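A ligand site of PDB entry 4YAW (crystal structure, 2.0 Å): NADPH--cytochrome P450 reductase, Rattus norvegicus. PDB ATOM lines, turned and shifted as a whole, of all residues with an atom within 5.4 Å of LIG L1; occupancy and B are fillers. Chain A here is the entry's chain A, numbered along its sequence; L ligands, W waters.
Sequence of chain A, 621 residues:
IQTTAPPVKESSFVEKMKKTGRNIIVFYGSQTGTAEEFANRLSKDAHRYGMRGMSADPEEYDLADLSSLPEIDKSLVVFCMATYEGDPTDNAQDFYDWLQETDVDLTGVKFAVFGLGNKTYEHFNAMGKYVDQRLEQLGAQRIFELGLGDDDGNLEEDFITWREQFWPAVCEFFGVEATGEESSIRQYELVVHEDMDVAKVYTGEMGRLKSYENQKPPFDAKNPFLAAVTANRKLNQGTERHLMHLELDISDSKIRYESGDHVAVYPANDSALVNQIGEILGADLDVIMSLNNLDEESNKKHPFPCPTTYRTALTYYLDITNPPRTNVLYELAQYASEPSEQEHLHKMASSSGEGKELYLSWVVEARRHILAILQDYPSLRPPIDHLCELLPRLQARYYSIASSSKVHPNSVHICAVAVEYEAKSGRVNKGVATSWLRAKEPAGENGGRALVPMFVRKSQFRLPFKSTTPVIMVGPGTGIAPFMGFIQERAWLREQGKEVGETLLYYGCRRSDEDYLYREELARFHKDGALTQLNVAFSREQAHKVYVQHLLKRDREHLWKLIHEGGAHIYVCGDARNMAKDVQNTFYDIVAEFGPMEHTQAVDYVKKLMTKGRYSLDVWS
The side-chain hydroxyl (OG1) of Thr 434 lies within hydrogen-bond range of an oxygen (O13) of LIG L1 (2.7 Å).
The backbone carbonyl oxygen (O) of Tyr 398 is in hydrogen-bond range of an oxygen (O9) of LIG L1 (2.7 Å).
An oxygen (O9) of LIG L1 lies within hydrogen-bond range of the backbone NH (N) of Tyr 398 (3.4 Å).
O6 of LIG L1 is in hydrogen-bond range of NH2 of Arg 367 (2.9 Å).
N of Val 432 sits at hydrogen-bond distance from O1 of LIG L1 (3.0 Å).
An oxygen (O7) of LIG L1 is in hydrogen-bond range of the backbone NH (N) of Val 417.
N of Ala 433 lies within hydrogen-bond range of O14 of LIG L1, 2.8 Å away.
N of Thr 434 is in hydrogen-bond range of O13 of LIG L1 (2.9 Å).
O of Cys 415 lies within hydrogen-bond range of N7 of LIG L1, 2.9 Å away.
O11 of LIG L1 is in hydrogen-bond range of OH of Tyr 399 (2.7 Å).
The guanidinium group of Arg 397 is in salt-bridge range of an oxygen (O14) of LIG L1 (2.9 Å).
N8 of LIG L1 is in hydrogen-bond range of OG of Ser 400, 3.4 Å away.
The backbone NH of Ser 400 is in hydrogen-bond range of an oxygen (O8) of LIG L1, at 2.9 Å.
N of Val 419 sits at hydrogen-bond distance from OG1 of Thr 434.
The guanidinium group of Arg 367 is in hydrogen-bond range of the side-chain amide oxygen of Asn 322, 3.4 Å away.
OG of Ser 435 lies within hydrogen-bond range of O of Gly 431 (2.7 Å).
OD2 of Asp 618 is in hydrogen-bond range of OG of Ser 400, at 2.7 Å.
NE of Arg 367 lies within hydrogen-bond range of OH of Tyr 421, at 3.1 Å.
N of Gly 431 is in hydrogen-bond range of O of Val 419 (2.9 Å).
Merely in contact with LIG L1: Gly 431, Ala 416, Trp 620, Tyr 421, His 262 and Val 419.
Hydrophobic or aromatic side chains that line LIG L1: His 262, Tyr 399, Ala 416, Val 419, Tyr 421, Val 432, Ala 433 and Trp 620.
Within 4 Å of LIG L1: His 262, Arg 367, Arg 397, Tyr 398, Tyr 399, Ser 400, Cys 415, Ala 416, Val 417, Val 419, Tyr 421, Gly 431, Val 432, Ala 433, Thr 434 and Trp 620.
Along chain A the residues within 4 Å of LIG L1 span positions 262 to 620.
Water W4 bridges an oxygen (O9) of LIG L1 and the backbone NH (N) of Tyr 398.
Water W6 lies within hydrogen-bond range of OH of Tyr 421, O4 of LIG L1 and NH1 of Arg 367.
Water W12 lies within hydrogen-bond range of an oxygen (O8) of LIG L1 (2.8 Å), the backbone NH (N) of Cys 415 (2.8 Å) and the backbone carbonyl oxygen (O) of Ser 400 (2.9 Å).
Water W8 lies within hydrogen-bond range of O2 of LIG L1 (3.0 Å) and ND2 of Asn 322 (3.2 Å).
Water W7 bridges O5 of LIG L1 (3.1 Å) and OD1 of Asn 322 (3.5 Å).
Water W3 lies within hydrogen-bond range of O of Lys 430 (2.7 Å) and O1 of LIG L1 (3.1 Å).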
ATOM      1  N   HIS A 262       9.199  11.275  -1.311  1.00  0.00           N
ATOM      2  CA  HIS A 262       9.211   9.912  -1.797  1.00  0.00           C
ATOM      3  C   HIS A 262       9.372   8.992  -0.608  1.00  0.00           C
ATOM      4  O   HIS A 262       9.911   9.385   0.425  1.00  0.00           O
ATOM      5  CB  HIS A 262      10.376   9.698  -2.769  1.00  0.00           C
ATOM      6  CG  HIS A 262      10.281  10.525  -4.021  1.00  0.00           C
ATOM      7  ND1 HIS A 262       9.335  10.295  -5.002  1.00  0.00           N
ATOM      8  CD2 HIS A 262      11.000  11.587  -4.442  1.00  0.00           C
ATOM      9  CE1 HIS A 262       9.476  11.175  -5.970  1.00  0.00           C
ATOM     10  NE2 HIS A 262      10.479  11.979  -5.646  1.00  0.00           N
ATOM     11  N   THR A 321      18.109 -10.116 -10.116  1.00  0.00           N
ATOM     12  CA  THR A 321      17.140  -9.991 -11.208  1.00  0.00           C
ATOM     13  C   THR A 321      17.550  -9.101 -12.365  1.00  0.00           C
ATOM     14  O   THR A 321      17.122  -9.325 -13.498  1.00  0.00           O
ATOM     15  CB  THR A 321      15.805  -9.487 -10.660  1.00  0.00           C
ATOM     16  OG1 THR A 321      16.030  -8.306  -9.899  1.00  0.00           O
ATOM     17  CG2 THR A 321      15.149 -10.546  -9.768  1.00  0.00           C
ATOM     18  N   ASN A 322      18.357  -8.088 -12.105  1.00  0.00           N
ATOM     19  CA  ASN A 322      18.805  -7.215 -13.180  1.00  0.00           C
ATOM     20  C   ASN A 322      19.884  -7.896 -14.013  1.00  0.00           C
ATOM     21  O   ASN A 322      20.583  -8.781 -13.514  1.00  0.00           O
ATOM     22  CB  ASN A 322      19.322  -5.895 -12.621  1.00  0.00           C
ATOM     23  CG  ASN A 322      18.218  -5.035 -12.060  1.00  0.00           C
ATOM     24  OD1 ASN A 322      17.169  -4.873 -12.695  1.00  0.00           O
ATOM     25  ND2 ASN A 322      18.435  -4.481 -10.874  1.00  0.00           N
ATOM     26  N   ARG A 367      16.899  -9.392 -21.166  1.00  0.00           N
ATOM     27  CA  ARG A 367      16.705  -9.245 -19.739  1.00  0.00           C
ATOM     28  C   ARG A 367      16.964 -10.536 -18.965  1.00  0.00           C
ATOM     29  O   ARG A 367      16.187 -10.927 -18.092  1.00  0.00           O
ATOM     30  CB  ARG A 367      15.291  -8.722 -19.444  1.00  0.00           C
ATOM     31  CG  ARG A 367      15.059  -7.278 -19.940  1.00  0.00           C
ATOM     32  CD  ARG A 367      15.749  -6.251 -19.047  1.00  0.00           C
ATOM     33  NE  ARG A 367      15.420  -6.501 -17.636  1.00  0.00           N
ATOM     34  CZ  ARG A 367      15.797  -5.733 -16.617  1.00  0.00           C
ATOM     35  NH1 ARG A 367      15.425  -6.075 -15.388  1.00  0.00           N
ATOM     36  NH2 ARG A 367      16.507  -4.627 -16.813  1.00  0.00           N
ATOM     37  N   ARG A 397      13.538   0.717  -3.338  1.00  0.00           N
ATOM     38  CA  ARG A 397      12.770   1.276  -4.447  1.00  0.00           C
ATOM     39  C   ARG A 397      12.027   2.523  -3.967  1.00  0.00           C
ATOM     40  O   ARG A 397      11.560   2.585  -2.824  1.00  0.00           O
ATOM     41  CB  ARG A 397      11.765   0.240  -4.990  1.00  0.00           C
ATOM     42  CG  ARG A 397      12.291  -0.653  -6.127  1.00  0.00           C
ATOM     43  CD  ARG A 397      13.409  -1.594  -5.701  1.00  0.00           C
ATOM     44  NE  ARG A 397      13.740  -2.506  -6.794  1.00  0.00           N
ATOM     45  CZ  ARG A 397      14.863  -3.227  -6.872  1.00  0.00           C
ATOM     46  NH1 ARG A 397      15.059  -4.014  -7.922  1.00  0.00           N
ATOM     47  NH2 ARG A 397      15.777  -3.145  -5.925  1.00  0.00           N
ATOM     48  N   TYR A 398      11.904   3.531  -4.832  1.00  0.00           N
ATOM     49  CA  TYR A 398      11.216   4.765  -4.471  1.00  0.00           C
ATOM     50  C   TYR A 398       9.801   4.889  -5.037  1.00  0.00           C
ATOM     51  O   TYR A 398       9.546   4.492  -6.172  1.00  0.00           O
ATOM     52  CB  TYR A 398      12.039   5.990  -4.912  1.00  0.00           C
ATOM     53  CG  TYR A 398      13.327   6.166  -4.133  1.00  0.00           C
ATOM     54  CD1 TYR A 398      14.422   5.341  -4.379  1.00  0.00           C
ATOM     55  CD2 TYR A 398      13.417   7.100  -3.115  1.00  0.00           C
ATOM     56  CE1 TYR A 398      15.586   5.444  -3.605  1.00  0.00           C
ATOM     57  CE2 TYR A 398      14.579   7.212  -2.337  1.00  0.00           C
ATOM     58  CZ  TYR A 398      15.654   6.386  -2.594  1.00  0.00           C
ATOM     59  OH  TYR A 398      16.788   6.493  -1.822  1.00  0.00           O
ATOM     60  N   TYR A 399       8.911   5.454  -4.237  1.00  0.00           N
ATOM     61  CA  TYR A 399       7.531   5.680  -4.627  1.00  0.00           C
ATOM     62  C   TYR A 399       7.122   7.082  -4.200  1.00  0.00           C
ATOM     63  O   TYR A 399       7.538   7.568  -3.150  1.00  0.00           O
ATOM     64  CB  TYR A 399       6.638   4.608  -4.011  1.00  0.00           C
ATOM     65  CG  TYR A 399       6.968   3.244  -4.548  1.00  0.00           C
ATOM     66  CD1 TYR A 399       6.465   2.816  -5.778  1.00  0.00           C
ATOM     67  CD2 TYR A 399       7.888   2.418  -3.894  1.00  0.00           C
ATOM     68  CE1 TYR A 399       6.868   1.615  -6.360  1.00  0.00           C
ATOM     69  CE2 TYR A 399       8.311   1.218  -4.466  1.00  0.00           C
ATOM     70  CZ  TYR A 399       7.803   0.823  -5.700  1.00  0.00           C
ATOM     71  OH  TYR A 399       8.250  -0.349  -6.274  1.00  0.00           O
ATOM     72  N   SER A 400       6.308   7.741  -5.021  1.00  0.00           N
ATOM     73  CA  SER A 400       5.870   9.096  -4.706  1.00  0.00           C
ATOM     74  C   SER A 400       4.725   8.986  -3.718  1.00  0.00           C
ATOM     75  O   SER A 400       3.648   8.482  -4.058  1.00  0.00           O
ATOM     76  CB  SER A 400       5.414   9.811  -5.990  1.00  0.00           C
ATOM     77  OG  SER A 400       6.428   9.804  -6.984  1.00  0.00           O
ATOM     78  N   CYS A 415       1.052   4.313  -4.599  1.00  0.00           N
ATOM     79  CA  CYS A 415       0.289   3.993  -5.794  1.00  0.00           C
ATOM     80  C   CYS A 415       1.298   3.453  -6.781  1.00  0.00           C
ATOM     81  O   CYS A 415       2.196   4.184  -7.208  1.00  0.00           O
ATOM     82  CB  CYS A 415      -0.378   5.256  -6.365  1.00  0.00           C
ATOM     83  SG  CYS A 415      -1.138   5.013  -7.993  1.00  0.00           S
ATOM     84  N   ALA A 416       1.159   2.188  -7.153  1.00  0.00           N
ATOM     85  CA  ALA A 416       2.106   1.569  -8.078  1.00  0.00           C
ATOM     86  C   ALA A 416       1.481   0.534  -8.996  1.00  0.00           C
ATOM     87  O   ALA A 416       0.403  -0.017  -8.725  1.00  0.00           O
ATOM     88  CB  ALA A 416       3.233   0.914  -7.292  1.00  0.00           C
ATOM     89  N   VAL A 417       2.174   0.263 -10.086  1.00  0.00           N
ATOM     90  CA  VAL A 417       1.735  -0.747 -11.040  1.00  0.00           C
ATOM     91  C   VAL A 417       2.688  -1.920 -10.824  1.00  0.00           C
ATOM     92  O   VAL A 417       3.892  -1.729 -10.686  1.00  0.00           O
ATOM     93  CB  VAL A 417       1.815  -0.208 -12.501  1.00  0.00           C
ATOM     94  CG1 VAL A 417       3.214   0.291 -12.795  1.00  0.00           C
ATOM     95  CG2 VAL A 417       1.418  -1.309 -13.474  1.00  0.00           C
ATOM     96  N   VAL A 419       5.044  -4.853 -11.694  1.00  0.00           N
ATOM     97  CA  VAL A 419       5.835  -5.172 -12.865  1.00  0.00           C
ATOM     98  C   VAL A 419       5.868  -6.677 -13.096  1.00  0.00           C
ATOM     99  O   VAL A 419       6.242  -7.445 -12.211  1.00  0.00           O
ATOM    100  CB  VAL A 419       7.279  -4.634 -12.746  1.00  0.00           C
ATOM    101  CG1 VAL A 419       8.110  -5.092 -13.954  1.00  0.00           C
ATOM    102  CG2 VAL A 419       7.259  -3.102 -12.685  1.00  0.00           C
ATOM    103  N   TYR A 421       6.397  -9.061 -16.822  1.00  0.00           N
ATOM    104  CA  TYR A 421       6.399  -9.094 -18.278  1.00  0.00           C
ATOM    105  C   TYR A 421       7.121 -10.281 -18.860  1.00  0.00           C
ATOM    106  O   TYR A 421       7.959 -10.901 -18.204  1.00  0.00           O
ATOM    107  CB  TYR A 421       7.023  -7.815 -18.839  1.00  0.00           C
ATOM    108  CG  TYR A 421       8.460  -7.625 -18.422  1.00  0.00           C
ATOM    109  CD1 TYR A 421       8.773  -7.142 -17.143  1.00  0.00           C
ATOM    110  CD2 TYR A 421       9.502  -7.975 -19.269  1.00  0.00           C
ATOM    111  CE1 TYR A 421      10.104  -7.023 -16.720  1.00  0.00           C
ATOM    112  CE2 TYR A 421      10.837  -7.861 -18.862  1.00  0.00           C
ATOM    113  CZ  TYR A 421      11.118  -7.396 -17.587  1.00  0.00           C
ATOM    114  OH  TYR A 421      12.432  -7.347 -17.160  1.00  0.00           O
ATOM    115  N   LYS A 430       9.672 -10.776 -13.027  1.00  0.00           N
ATOM    116  CA  LYS A 430       8.837 -10.135 -12.019  1.00  0.00           C
ATOM    117  C   LYS A 430       9.600  -8.998 -11.341  1.00  0.00           C
ATOM    118  O   LYS A 430      10.787  -9.126 -11.032  1.00  0.00           O
ATOM    119  CB  LYS A 430       8.426 -11.157 -10.954  1.00  0.00           C
ATOM    120  CG  LYS A 430       7.679 -12.388 -11.466  1.00  0.00           C
ATOM    121  CD  LYS A 430       6.207 -12.090 -11.750  1.00  0.00           C
ATOM    122  CE  LYS A 430       5.460 -11.686 -10.476  1.00  0.00           C
ATOM    123  NZ  LYS A 430       5.495 -12.764  -9.427  1.00  0.00           N
ATOM    124  N   GLY A 431       8.905  -7.874 -11.142  1.00  0.00           N
ATOM    125  CA  GLY A 431       9.516  -6.739 -10.477  1.00  0.00           C
ATOM    126  C   GLY A 431       9.733  -7.092  -9.025  1.00  0.00           C
ATOM    127  O   GLY A 431       8.818  -7.594  -8.353  1.00  0.00           O
ATOM    128  N   VAL A 432      10.930  -6.849  -8.522  1.00  0.00           N
ATOM    129  CA  VAL A 432      11.250  -7.179  -7.132  1.00  0.00           C
ATOM    130  C   VAL A 432      10.363  -6.500  -6.079  1.00  0.00           C
ATOM    131  O   VAL A 432       9.669  -7.180  -5.321  1.00  0.00           O
ATOM    132  CB  VAL A 432      12.735  -6.866  -6.823  1.00  0.00           C
ATOM    133  CG1 VAL A 432      13.049  -7.197  -5.367  1.00  0.00           C
ATOM    134  CG2 VAL A 432      13.634  -7.685  -7.766  1.00  0.00           C
ATOM    135  N   ALA A 433      10.391  -5.183  -6.021  1.00  0.00           N
ATOM    136  CA  ALA A 433       9.596  -4.460  -5.031  1.00  0.00           C
ATOM    137  C   ALA A 433       8.076  -4.566  -5.209  1.00  0.00           C
ATOM    138  O   ALA A 433       7.359  -4.761  -4.228  1.00  0.00           O
ATOM    139  CB  ALA A 433      10.003  -2.986  -4.997  1.00  0.00           C
ATOM    140  N   THR A 434       7.595  -4.436  -6.441  1.00  0.00           N
ATOM    141  CA  THR A 434       6.145  -4.491  -6.653  1.00  0.00           C
ATOM    142  C   THR A 434       5.533  -5.873  -6.430  1.00  0.00           C
ATOM    143  O   THR A 434       4.393  -5.970  -5.975  1.00  0.00           O
ATOM    144  CB  THR A 434       5.752  -3.947  -8.059  1.00  0.00           C
ATOM    145  OG1 THR A 434       6.432  -4.689  -9.077  1.00  0.00           O
ATOM    146  CG2 THR A 434       6.114  -2.466  -8.179  1.00  0.00           C
ATOM    147  N   SER A 435       6.260  -6.943  -6.736  1.00  0.00           N
ATOM    148  CA  SER A 435       5.744  -8.288  -6.518  1.00  0.00           C
ATOM    149  C   SER A 435       5.654  -8.511  -5.006  1.00  0.00           C
ATOM    150  O   SER A 435       4.685  -9.073  -4.490  1.00  0.00           O
ATOM    151  CB  SER A 435       6.681  -9.350  -7.119  1.00  0.00           C
ATOM    152  OG  SER A 435       6.710  -9.262  -8.528  1.00  0.00           O
ATOM    153  N   THR A 478       0.152   6.073 -13.182  1.00  0.00           N
ATOM    154  CA  THR A 478       0.602   6.115 -11.802  1.00  0.00           C
ATOM    155  C   THR A 478       1.212   7.488 -11.468  1.00  0.00           C
ATOM    156  O   THR A 478       1.608   7.743 -10.321  1.00  0.00           O
ATOM    157  CB  THR A 478       1.626   5.002 -11.518  1.00  0.00           C
ATOM    158  OG1 THR A 478       2.775   5.174 -12.361  1.00  0.00           O
ATOM    159  CG2 THR A 478       1.015   3.636 -11.773  1.00  0.00           C
ATOM    160  N   ALA A 481      -0.084   9.679  -8.437  1.00  0.00           N
ATOM    161  CA  ALA A 481       0.331   9.458  -7.042  1.00  0.00           C
ATOM    162  C   ALA A 481       0.520  10.647  -6.101  1.00  0.00           C
ATOM    163  O   ALA A 481      -0.223  10.808  -5.140  1.00  0.00           O
ATOM    164  CB  ALA A 481       1.589   8.589  -7.027  1.00  0.00           C
ATOM    165  N   ASP A 618       8.512  15.081 -11.299  1.00  0.00           N
ATOM    166  CA  ASP A 618       8.640  13.893 -10.475  1.00  0.00           C
ATOM    167  C   ASP A 618       8.459  12.787 -11.498  1.00  0.00           C
ATOM    168  O   ASP A 618       7.475  12.069 -11.509  1.00  0.00           O
ATOM    169  CB  ASP A 618       7.524  13.831  -9.413  1.00  0.00           C
ATOM    170  CG  ASP A 618       7.638  12.606  -8.521  1.00  0.00           C
ATOM    171  OD1 ASP A 618       8.594  11.821  -8.695  1.00  0.00           O
ATOM    172  OD2 ASP A 618       6.779  12.406  -7.635  1.00  0.00           O
ATOM    173  N   VAL A 619       9.434  12.682 -12.387  1.00  0.00           N
ATOM    174  CA  VAL A 619       9.375  11.704 -13.447  1.00  0.00           C
ATOM    175  C   VAL A 619      10.406  10.599 -13.280  1.00  0.00           C
ATOM    176  O   VAL A 619      11.456  10.787 -12.687  1.00  0.00           O
ATOM    177  CB  VAL A 619       9.558  12.394 -14.826  1.00  0.00           C
ATOM    178  CG1 VAL A 619       8.386  13.332 -15.086  1.00  0.00           C
ATOM    179  CG2 VAL A 619      10.865  13.181 -14.848  1.00  0.00           C
ATOM    180  N   TRP A 620      10.050   9.437 -13.801  1.00  0.00           N
ATOM    181  CA  TRP A 620      10.923   8.275 -13.713  1.00  0.00           C
ATOM    182  C   TRP A 620      10.715   7.414 -14.947  1.00  0.00           C
ATOM    183  O   TRP A 620       9.804   7.661 -15.738  1.00  0.00           O
ATOM    184  CB  TRP A 620      10.598   7.505 -12.426  1.00  0.00           C
ATOM    185  CG  TRP A 620       9.208   6.934 -12.337  1.00  0.00           C
ATOM    186  CD1 TRP A 620       8.778   5.747 -12.869  1.00  0.00           C
ATOM    187  CD2 TRP A 620       8.059   7.518 -11.692  1.00  0.00           C
ATOM    188  NE1 TRP A 620       7.435   5.561 -12.599  1.00  0.00           N
ATOM    189  CE2 TRP A 620       6.972   6.626 -11.877  1.00  0.00           C
ATOM    190  CE3 TRP A 620       7.846   8.703 -10.978  1.00  0.00           C
ATOM    191  CZ2 TRP A 620       5.689   6.899 -11.375  1.00  0.00           C
ATOM    192  CZ3 TRP A 620       6.565   8.966 -10.479  1.00  0.00           C
ATOM    193  CH2 TRP A 620       5.505   8.062 -10.673  1.00  0.00           C
ATOM    194  N   SER A 621      11.551   6.401 -15.112  1.00  0.00           N
ATOM    195  CA  SER A 621      11.480   5.491 -16.255  1.00  0.00           C
ATOM    196  C   SER A 621      10.639   4.247 -15.967  1.00  0.00           C
ATOM    197  O   SER A 621       9.609   4.366 -15.261  1.00  0.00           O
ATOM    198  CB  SER A 621      12.885   5.087 -16.690  1.00  0.00           C
ATOM    199  OG  SER A 621      13.633   4.657 -15.561  1.00  0.00           O
ATOM    200  OXT SER A 621      11.013   3.151 -16.463  1.00  0.00           O
HETATM  201  P1  LIG L   1      12.456  -4.030 -10.799  1.00  0.00           P
HETATM  202  O1  LIG L   1      12.812  -5.398 -10.373  1.00  0.00           O
HETATM  203  O2  LIG L   1      13.196  -2.881 -10.242  1.00  0.00           O
HETATM  204  O3  LIG L   1      12.501  -3.969 -12.413  1.00  0.00           O
HETATM  205  C1  LIG L   1      12.436  -2.713 -13.099  1.00  0.00           C
HETATM  206  C2  LIG L   1      13.045  -2.886 -14.490  1.00  0.00           C
HETATM  207  O4  LIG L   1      12.376  -3.917 -15.223  1.00  0.00           O
HETATM  208  C3  LIG L   1      12.835  -1.654 -15.347  1.00  0.00           C
HETATM  209  O5  LIG L   1      13.791  -0.651 -14.973  1.00  0.00           O
HETATM  210  C4  LIG L   1      13.228  -2.256 -16.684  1.00  0.00           C
HETATM  211  O6  LIG L   1      14.659  -2.363 -16.783  1.00  0.00           O
HETATM  212  C5  LIG L   1      12.609  -3.645 -16.609  1.00  0.00           C
HETATM  213  N1  LIG L   1      11.281  -3.684 -17.275  1.00  0.00           N
HETATM  214  C6  LIG L   1      10.001  -3.229 -16.701  1.00  0.00           C
HETATM  215  N2  LIG L   1       9.076  -3.580 -17.790  1.00  0.00           N
HETATM  216  C7  LIG L   1       9.771  -4.108 -18.791  1.00  0.00           C
HETATM  217  C8  LIG L   1       9.338  -4.569 -19.964  1.00  0.00           C
HETATM  218  N3  LIG L   1       8.031  -4.476 -20.187  1.00  0.00           N
HETATM  219  N4  LIG L   1      10.169  -5.013 -20.917  1.00  0.00           N
HETATM  220  C9  LIG L   1      11.551  -4.986 -20.671  1.00  0.00           C
HETATM  221  N5  LIG L   1      11.974  -4.480 -19.446  1.00  0.00           N
HETATM  222  C10 LIG L   1      11.075  -4.061 -18.533  1.00  0.00           C
HETATM  223  N6  LIG L   1       6.682   3.607  -9.665  1.00  0.00           N
HETATM  224  C11 LIG L   1       5.319   3.550  -9.374  1.00  0.00           C
HETATM  225  O7  LIG L   1       4.635   2.649  -9.852  1.00  0.00           O
HETATM  226  N7  LIG L   1       4.731   4.554  -8.591  1.00  0.00           N
HETATM  227  C12 LIG L   1       5.509   5.619  -8.112  1.00  0.00           C
HETATM  228  O8  LIG L   1       5.014   6.410  -7.302  1.00  0.00           O
HETATM  229  C13 LIG L   1       6.854   5.678  -8.426  1.00  0.00           C
HETATM  230  N8  LIG L   1       7.570   6.785  -8.122  1.00  0.00           N
HETATM  231  C14 LIG L   1       8.879   6.831  -8.423  1.00  0.00           C
HETATM  232  C15 LIG L   1       9.625   7.945  -8.051  1.00  0.00           C
HETATM  233  C16 LIG L   1      10.987   7.983  -8.318  1.00  0.00           C
HETATM  234  C17 LIG L   1      11.761   9.019  -7.789  1.00  0.00           C
HETATM  235  C18 LIG L   1      11.604   6.921  -8.967  1.00  0.00           C
HETATM  236  C19 LIG L   1      12.969   6.950  -9.238  1.00  0.00           C
HETATM  237  C20 LIG L   1      10.857   5.803  -9.326  1.00  0.00           C
HETATM  238  C21 LIG L   1       9.499   5.745  -9.027  1.00  0.00           C
HETATM  239  N9  LIG L   1       8.779   4.643  -9.316  1.00  0.00           N
HETATM  240  C22 LIG L   1       7.446   4.683  -9.199  1.00  0.00           C
HETATM  241  C23 LIG L   1       9.413   3.456  -9.932  1.00  0.00           C
HETATM  242  C24 LIG L   1       9.830   2.495  -8.816  1.00  0.00           C
HETATM  243  O9  LIG L   1      10.870   3.093  -8.031  1.00  0.00           O
HETATM  244  C25 LIG L   1      10.310   1.132  -9.340  1.00  0.00           C
HETATM  245  O10 LIG L   1      11.333   1.308 -10.327  1.00  0.00           O
HETATM  246  C26 LIG L   1       9.134   0.346  -9.922  1.00  0.00           C
HETATM  247  O11 LIG L   1       8.105   0.211  -8.936  1.00  0.00           O
HETATM  248  C27 LIG L   1       9.610  -1.046 -10.359  1.00  0.00           C
HETATM  249  O12 LIG L   1      10.330  -1.660  -9.284  1.00  0.00           O
HETATM  250  P2  LIG L   1      10.361  -3.252  -9.085  1.00  0.00           P
HETATM  251  O13 LIG L   1       8.982  -3.741  -8.906  1.00  0.00           O
HETATM  252  O14 LIG L   1      11.366  -3.556  -8.045  1.00  0.00           O
HETATM  253  O15 LIG L   1      10.884  -3.791 -10.512  1.00  0.00           O
HETATM  254  N1  LG2 L   2      21.054  11.893 -14.801  1.00  0.00           N
HETATM  255  C1  LG2 L   2      21.464  13.103 -15.247  1.00  0.00           C
HETATM  256  O1  LG2 L   2      22.373  13.194 -16.059  1.00  0.00           O
HETATM  257  N2  LG2 L   2      20.809  14.201 -14.741  1.00  0.00           N
HETATM  258  C2  LG2 L   2      19.758  14.212 -13.819  1.00  0.00           C
HETATM  259  O2  LG2 L   2      19.331  15.326 -13.521  1.00  0.00           O
HETATM  260  C3  LG2 L   2      19.315  12.951 -13.343  1.00  0.00           C
HETATM  261  N3  LG2 L   2      18.239  12.933 -12.420  1.00  0.00           N
HETATM  262  C4  LG2 L   2      17.859  11.649 -12.019  1.00  0.00           C
HETATM  263  C5  LG2 L   2      16.767  11.592 -11.089  1.00  0.00           C
HETATM  264  C6  LG2 L   2      16.272  10.357 -10.595  1.00  0.00           C
HETATM  265  C7  LG2 L   2      15.093  10.464  -9.603  1.00  0.00           C
HETATM  266  C8  LG2 L   2      16.891   9.067 -11.038  1.00  0.00           C
HETATM  267  C9  LG2 L   2      16.501   7.802 -10.640  1.00  0.00           C
HETATM  268  C10 LG2 L   2      17.945   9.105 -11.942  1.00  0.00           C
HETATM  269  C11 LG2 L   2      18.466  10.374 -12.451  1.00  0.00           C
HETATM  270  N4  LG2 L   2      19.581  10.501 -13.414  1.00  0.00           N
HETATM  271  C12 LG2 L   2      20.009  11.830 -13.882  1.00  0.00           C
HETATM  272  C13 LG2 L   2      20.241   9.310 -13.899  1.00  0.00           C
HETATM  273  C14 LG2 L   2      21.396   8.805 -12.988  1.00  0.00           C
HETATM  274  O3  LG2 L   2      22.422   9.869 -12.847  1.00  0.00           O
HETATM  275  C15 LG2 L   2      21.997   7.554 -13.600  1.00  0.00           C
HETATM  276  O4  LG2 L   2      20.940   6.577 -13.667  1.00  0.00           O
HETATM  277  C16 LG2 L   2      23.184   7.081 -12.696  1.00  0.00           C
HETATM  278  O5  LG2 L   2      23.641   5.913 -13.441  1.00  0.00           O
HETATM  279  C17 LG2 L   2      22.790   6.588 -11.319  1.00  0.00           C
HETATM  280  O6  LG2 L   2      23.982   6.208 -10.532  1.00  0.00           O
HETATM  281  P1  LG2 L   2      24.022   5.625  -9.079  1.00  0.00           P
HETATM  282  O7  LG2 L   2      23.413   4.264  -9.083  1.00  0.00           O
HETATM  283  O8  LG2 L   2      23.399   6.747  -8.190  1.00  0.00           O
HETATM  284  O9  LG2 L   2      25.606   5.477  -8.870  1.00  0.00           O
HETATM  285  O   HOH W   1      11.319   1.258 -12.971  1.00  0.00           O
HETATM  286  O   HOH W   2       6.688  -5.761 -22.185  1.00  0.00           O
HETATM  287  O   HOH W   3      12.751  -7.822 -12.336  1.00  0.00           O
HETATM  288  O   HOH W   4      13.352   3.307  -7.481  1.00  0.00           O
HETATM  289  O   HOH W   5      15.355  -6.057 -11.148  1.00  0.00           O
HETATM  290  O   HOH W   6      12.859  -6.514 -14.645  1.00  0.00           O
HETATM  291  O   HOH W   7      16.290  -1.560 -13.354  1.00  0.00           O
HETATM  292  O   HOH W   8      16.061  -2.392 -10.875  1.00  0.00           O
HETATM  293  O   HOH W   9       6.392  -2.971 -16.840  1.00  0.00           O
HETATM  294  O   HOH W  10      15.119  -4.081 -20.681  1.00  0.00           O
HETATM  295  O   HOH W  11       5.712   0.396 -10.407  1.00  0.00           O
HETATM  296  O   HOH W  12       3.351   5.822  -5.145  1.00  0.00           O
HETATM  297  O   HOH W  13      13.422  -0.216  -9.820  1.00  0.00           O
HETATM  298  O   HOH W  14      13.218   3.651 -10.899  1.00  0.00           O
